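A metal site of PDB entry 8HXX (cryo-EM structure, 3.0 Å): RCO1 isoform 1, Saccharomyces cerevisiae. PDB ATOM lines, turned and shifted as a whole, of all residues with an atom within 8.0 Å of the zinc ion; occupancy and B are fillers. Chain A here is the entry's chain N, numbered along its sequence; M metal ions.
Four residues have an atom within 4 Å of the zinc ion: Cys 417, Cys 420, His 448 and Cys 451.
N of Lys 419 sits close to SG of Cys 417 (3.7 Å). The backbone carbonyl oxygen (O) of Gln 422 is in hydrogen-bond range of the backbone NH (N) of Cys 417. The side-chain sulfur of Cys 420 lies close to the backbone carbonyl oxygen of Gln 422, at 3.5 Å.
The zinc ion is bound by a ring nitrogen (ND1) of His 448 (2.1 Å), the side-chain sulfur of Cys 451 (2.3 Å), the side-chain sulfur of Cys 417 (2.3 Å) and the side-chain sulfur of Cys 420 (2.3 Å).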
ATOM      1  N   LEU A 415      -4.599  14.998  17.745  1.00  0.00           N
ATOM      2  CA  LEU A 415      -3.201  14.601  17.898  1.00  0.00           C
ATOM      3  C   LEU A 415      -2.514  15.581  18.837  1.00  0.00           C
ATOM      4  O   LEU A 415      -2.105  16.667  18.433  1.00  0.00           O
ATOM      5  CB  LEU A 415      -2.502  14.558  16.542  1.00  0.00           C
ATOM      6  CG  LEU A 415      -2.995  13.511  15.540  1.00  0.00           C
ATOM      7  CD1 LEU A 415      -2.047  13.428  14.364  1.00  0.00           C
ATOM      8  CD2 LEU A 415      -3.126  12.152  16.213  1.00  0.00           C
ATOM      9  N   ILE A 416      -2.388  15.192  20.106  1.00  0.00           N
ATOM     10  CA  ILE A 416      -1.718  16.018  21.102  1.00  0.00           C
ATOM     11  C   ILE A 416      -0.216  15.873  20.910  1.00  0.00           C
ATOM     12  O   ILE A 416       0.306  14.753  20.952  1.00  0.00           O
ATOM     13  CB  ILE A 416      -2.136  15.621  22.523  1.00  0.00           C
ATOM     14  CG1 ILE A 416      -3.626  15.878  22.742  1.00  0.00           C
ATOM     15  CG2 ILE A 416      -1.283  16.342  23.552  1.00  0.00           C
ATOM     16  CD1 ILE A 416      -3.974  17.337  22.944  1.00  0.00           C
ATOM     17  N   CYS A 417       0.478  16.979  20.688  1.00  0.00           N
ATOM     18  CA  CYS A 417       1.927  16.955  20.588  1.00  0.00           C
ATOM     19  C   CYS A 417       2.539  16.554  21.922  1.00  0.00           C
ATOM     20  O   CYS A 417       1.995  16.840  22.983  1.00  0.00           O
ATOM     21  CB  CYS A 417       2.472  18.317  20.149  1.00  0.00           C
ATOM     22  SG  CYS A 417       4.272  18.394  20.164  1.00  0.00           S
ATOM     23  N   TYR A 418       3.668  15.849  21.852  1.00  0.00           N
ATOM     24  CA  TYR A 418       4.245  15.268  23.063  1.00  0.00           C
ATOM     25  C   TYR A 418       4.863  16.326  23.965  1.00  0.00           C
ATOM     26  O   TYR A 418       4.677  16.292  25.186  1.00  0.00           O
ATOM     27  CB  TYR A 418       5.269  14.201  22.694  1.00  0.00           C
ATOM     28  CG  TYR A 418       5.901  13.569  23.914  1.00  0.00           C
ATOM     29  CD1 TYR A 418       5.186  12.650  24.681  1.00  0.00           C
ATOM     30  CD2 TYR A 418       7.186  13.893  24.307  1.00  0.00           C
ATOM     31  CE1 TYR A 418       5.753  12.085  25.802  1.00  0.00           C
ATOM     32  CE2 TYR A 418       7.753  13.328  25.428  1.00  0.00           C
ATOM     33  CZ  TYR A 418       7.036  12.417  26.165  1.00  0.00           C
ATOM     34  OH  TYR A 418       7.606  11.861  27.275  1.00  0.00           O
ATOM     35  N   LYS A 419       5.599  17.270  23.387  1.00  0.00           N
ATOM     36  CA  LYS A 419       6.357  18.210  24.219  1.00  0.00           C
ATOM     37  C   LYS A 419       5.452  19.308  24.786  1.00  0.00           C
ATOM     38  O   LYS A 419       5.430  19.528  25.998  1.00  0.00           O
ATOM     39  CB  LYS A 419       7.499  18.825  23.410  1.00  0.00           C
ATOM     40  CG  LYS A 419       8.266  19.897  24.156  1.00  0.00           C
ATOM     41  CD  LYS A 419       9.680  20.039  23.621  1.00  0.00           C
ATOM     42  CE  LYS A 419      10.545  18.866  24.038  1.00  0.00           C
ATOM     43  NZ  LYS A 419      10.610  18.721  25.522  1.00  0.00           N
ATOM     44  N   CYS A 420       4.706  19.992  23.930  1.00  0.00           N
ATOM     45  CA  CYS A 420       3.878  21.103  24.387  1.00  0.00           C
ATOM     46  C   CYS A 420       2.569  20.655  25.015  1.00  0.00           C
ATOM     47  O   CYS A 420       1.899  21.485  25.636  1.00  0.00           O
ATOM     48  CB  CYS A 420       3.594  22.059  23.228  1.00  0.00           C
ATOM     49  SG  CYS A 420       2.614  21.354  21.890  1.00  0.00           S
ATOM     50  N   ASN A 421       2.212  19.375  24.867  1.00  0.00           N
ATOM     51  CA  ASN A 421       0.963  18.788  25.382  1.00  0.00           C
ATOM     52  C   ASN A 421      -0.272  19.530  24.870  1.00  0.00           C
ATOM     53  O   ASN A 421      -1.262  19.676  25.582  1.00  0.00           O
ATOM     54  CB  ASN A 421       0.963  18.719  26.910  1.00  0.00           C
ATOM     55  CG  ASN A 421       1.440  17.379  27.426  1.00  0.00           C
ATOM     56  OD1 ASN A 421       1.513  16.406  26.685  1.00  0.00           O
ATOM     57  ND2 ASN A 421       1.786  17.332  28.712  1.00  0.00           N
ATOM     58  N   GLN A 422      -0.205  20.001  23.628  1.00  0.00           N
ATOM     59  CA  GLN A 422      -1.281  20.771  23.019  1.00  0.00           C
ATOM     60  C   GLN A 422      -1.382  20.411  21.550  1.00  0.00           C
ATOM     61  O   GLN A 422      -0.444  19.884  20.947  1.00  0.00           O
ATOM     62  CB  GLN A 422      -1.048  22.287  23.161  1.00  0.00           C
ATOM     63  CG  GLN A 422      -1.298  22.846  24.542  1.00  0.00           C
ATOM     64  CD  GLN A 422      -0.862  24.296  24.660  1.00  0.00           C
ATOM     65  OE1 GLN A 422      -0.286  24.705  25.662  1.00  0.00           O
ATOM     66  NE2 GLN A 422      -1.137  25.080  23.614  1.00  0.00           N
ATOM     67  N   THR A 423      -2.543  20.691  20.966  1.00  0.00           N
ATOM     68  CA  THR A 423      -2.726  20.653  19.522  1.00  0.00           C
ATOM     69  C   THR A 423      -3.179  22.034  19.061  1.00  0.00           C
ATOM     70  O   THR A 423      -4.292  22.467  19.377  1.00  0.00           O
ATOM     71  CB  THR A 423      -3.691  19.546  19.088  1.00  0.00           C
ATOM     72  OG1 THR A 423      -4.109  19.760  17.733  1.00  0.00           O
ATOM     73  CG2 THR A 423      -4.912  19.447  20.019  1.00  0.00           C
ATOM     74  N   ARG A 424      -2.304  22.738  18.353  1.00  0.00           N
ATOM     75  CA  ARG A 424      -2.592  24.099  17.897  1.00  0.00           C
ATOM     76  C   ARG A 424      -3.274  23.996  16.534  1.00  0.00           C
ATOM     77  O   ARG A 424      -2.641  24.052  15.479  1.00  0.00           O
ATOM     78  CB  ARG A 424      -1.323  24.933  17.856  1.00  0.00           C
ATOM     79  CG  ARG A 424      -0.390  24.647  19.024  1.00  0.00           C
ATOM     80  CD  ARG A 424      -0.655  25.573  20.188  1.00  0.00           C
ATOM     81  NE  ARG A 424      -0.303  26.955  19.885  1.00  0.00           N
ATOM     82  CZ  ARG A 424       0.911  27.463  20.005  1.00  0.00           C
ATOM     83  NH1 ARG A 424       1.930  26.723  20.432  1.00  0.00           N
ATOM     84  NH2 ARG A 424       1.119  28.738  19.695  1.00  0.00           N
ATOM     85  N   ARG A 435      -0.049  25.639  14.670  1.00  0.00           N
ATOM     86  CA  ARG A 435       1.303  25.114  14.619  1.00  0.00           C
ATOM     87  C   ARG A 435       1.274  23.765  13.906  1.00  0.00           C
ATOM     88  O   ARG A 435       0.386  22.948  14.148  1.00  0.00           O
ATOM     89  CB  ARG A 435       1.898  24.970  16.015  1.00  0.00           C
ATOM     90  CG  ARG A 435       2.008  26.281  16.772  1.00  0.00           C
ATOM     91  CD  ARG A 435       3.052  27.183  16.166  1.00  0.00           C
ATOM     92  NE  ARG A 435       3.010  28.526  16.731  1.00  0.00           N
ATOM     93  CZ  ARG A 435       2.300  29.526  16.241  1.00  0.00           C
ATOM     94  NH1 ARG A 435       1.543  29.365  15.163  1.00  0.00           N
ATOM     95  NH2 ARG A 435       2.338  30.706  16.841  1.00  0.00           N
ATOM     96  N   LEU A 436       2.257  23.544  13.032  1.00  0.00           N
ATOM     97  CA  LEU A 436       2.276  22.339  12.215  1.00  0.00           C
ATOM     98  C   LEU A 436       2.660  21.139  13.067  1.00  0.00           C
ATOM     99  O   LEU A 436       3.468  21.242  13.992  1.00  0.00           O
ATOM    100  CB  LEU A 436       3.268  22.487  11.067  1.00  0.00           C
ATOM    101  CG  LEU A 436       3.041  23.684  10.138  1.00  0.00           C
ATOM    102  CD1 LEU A 436       3.981  24.830  10.516  1.00  0.00           C
ATOM    103  CD2 LEU A 436       3.215  23.305   8.690  1.00  0.00           C
ATOM    104  N   ILE A 437       2.060  19.991  12.757  1.00  0.00           N
ATOM    105  CA  ILE A 437       2.286  18.773  13.522  1.00  0.00           C
ATOM    106  C   ILE A 437       2.510  17.611  12.566  1.00  0.00           C
ATOM    107  O   ILE A 437       1.886  17.539  11.497  1.00  0.00           O
ATOM    108  CB  ILE A 437       1.119  18.502  14.506  1.00  0.00           C
ATOM    109  CG1 ILE A 437       1.444  17.347  15.453  1.00  0.00           C
ATOM    110  CG2 ILE A 437      -0.200  18.266  13.780  1.00  0.00           C
ATOM    111  CD1 ILE A 437       0.670  17.386  16.744  1.00  0.00           C
ATOM    112  N   PRO A 446       2.822  12.032  17.872  1.00  0.00           N
ATOM    113  CA  PRO A 446       2.713  13.323  17.181  1.00  0.00           C
ATOM    114  C   PRO A 446       3.612  14.378  17.826  1.00  0.00           C
ATOM    115  O   PRO A 446       3.636  14.530  19.048  1.00  0.00           O
ATOM    116  CB  PRO A 446       1.233  13.690  17.324  1.00  0.00           C
ATOM    117  CG  PRO A 446       0.681  12.803  18.383  1.00  0.00           C
ATOM    118  CD  PRO A 446       1.694  11.789  18.795  1.00  0.00           C
ATOM    119  N   TRP A 447       4.337  15.098  16.976  1.00  0.00           N
ATOM    120  CA  TRP A 447       5.236  16.132  17.457  1.00  0.00           C
ATOM    121  C   TRP A 447       5.064  17.383  16.638  1.00  0.00           C
ATOM    122  O   TRP A 447       4.936  17.311  15.428  1.00  0.00           O
ATOM    123  CB  TRP A 447       6.684  15.668  17.313  1.00  0.00           C
ATOM    124  CG  TRP A 447       7.189  14.787  18.380  1.00  0.00           C
ATOM    125  CD1 TRP A 447       7.071  13.432  18.456  1.00  0.00           C
ATOM    126  CD2 TRP A 447       7.945  15.187  19.527  1.00  0.00           C
ATOM    127  NE1 TRP A 447       7.686  12.969  19.585  1.00  0.00           N
ATOM    128  CE2 TRP A 447       8.232  14.024  20.268  1.00  0.00           C
ATOM    129  CE3 TRP A 447       8.401  16.412  20.002  1.00  0.00           C
ATOM    130  CZ2 TRP A 447       8.960  14.055  21.447  1.00  0.00           C
ATOM    131  CZ3 TRP A 447       9.121  16.447  21.183  1.00  0.00           C
ATOM    132  CH2 TRP A 447       9.383  15.271  21.899  1.00  0.00           C
ATOM    133  N   HIS A 448       5.048  18.530  17.292  1.00  0.00           N
ATOM    134  CA  HIS A 448       4.963  19.807  16.597  1.00  0.00           C
ATOM    135  C   HIS A 448       6.246  20.078  15.823  1.00  0.00           C
ATOM    136  O   HIS A 448       7.316  19.585  16.164  1.00  0.00           O
ATOM    137  CB  HIS A 448       4.696  20.940  17.584  1.00  0.00           C
ATOM    138  CG  HIS A 448       3.242  21.183  17.846  1.00  0.00           C
ATOM    139  ND1 HIS A 448       2.741  21.382  19.114  1.00  0.00           N
ATOM    140  CD2 HIS A 448       2.181  21.262  17.007  1.00  0.00           C
ATOM    141  CE1 HIS A 448       1.439  21.567  19.045  1.00  0.00           C
ATOM    142  NE2 HIS A 448       1.070  21.504  17.776  1.00  0.00           N
ATOM    143  N   LEU A 449       6.188  20.858  14.759  1.00  0.00           N
ATOM    144  CA  LEU A 449       7.429  21.128  14.067  1.00  0.00           C
ATOM    145  C   LEU A 449       8.286  22.160  14.793  1.00  0.00           C
ATOM    146  O   LEU A 449       9.437  22.343  14.450  1.00  0.00           O
ATOM    147  CB  LEU A 449       7.164  21.581  12.634  1.00  0.00           C
ATOM    148  CG  LEU A 449       6.942  20.488  11.602  1.00  0.00           C
ATOM    149  CD1 LEU A 449       8.206  19.663  11.442  1.00  0.00           C
ATOM    150  CD2 LEU A 449       5.773  19.599  11.979  1.00  0.00           C
ATOM    151  N   ASP A 450       7.733  22.843  15.799  1.00  0.00           N
ATOM    152  CA  ASP A 450       8.545  23.779  16.568  1.00  0.00           C
ATOM    153  C   ASP A 450       9.080  23.174  17.860  1.00  0.00           C
ATOM    154  O   ASP A 450      10.115  23.635  18.359  1.00  0.00           O
ATOM    155  CB  ASP A 450       7.735  25.025  16.917  1.00  0.00           C
ATOM    156  CG  ASP A 450       7.072  25.641  15.704  1.00  0.00           C
ATOM    157  OD1 ASP A 450       7.350  25.202  14.572  1.00  0.00           O
ATOM    158  OD2 ASP A 450       6.273  26.574  15.892  1.00  0.00           O
ATOM    159  N   CYS A 451       8.386  22.183  18.429  1.00  0.00           N
ATOM    160  CA  CYS A 451       8.853  21.562  19.666  1.00  0.00           C
ATOM    161  C   CYS A 451      10.139  20.784  19.428  1.00  0.00           C
ATOM    162  O   CYS A 451      11.118  20.930  20.170  1.00  0.00           O
ATOM    163  CB  CYS A 451       7.763  20.657  20.230  1.00  0.00           C
ATOM    164  SG  CYS A 451       6.316  21.561  20.851  1.00  0.00           S
ATOM    165  N   VAL A 452      10.162  19.937  18.400  1.00  0.00           N
ATOM    166  CA  VAL A 452      11.420  19.439  17.847  1.00  0.00           C
ATOM    167  C   VAL A 452      11.846  20.452  16.794  1.00  0.00           C
ATOM    168  O   VAL A 452      11.012  20.931  16.012  1.00  0.00           O
ATOM    169  CB  VAL A 452      11.273  17.996  17.316  1.00  0.00           C
ATOM    170  CG1 VAL A 452      10.225  17.886  16.220  1.00  0.00           C
ATOM    171  CG2 VAL A 452      12.614  17.475  16.827  1.00  0.00           C
HETATM  172 ZN    ZN M   1       4.227  20.697  20.368  1.00  0.00          ZN
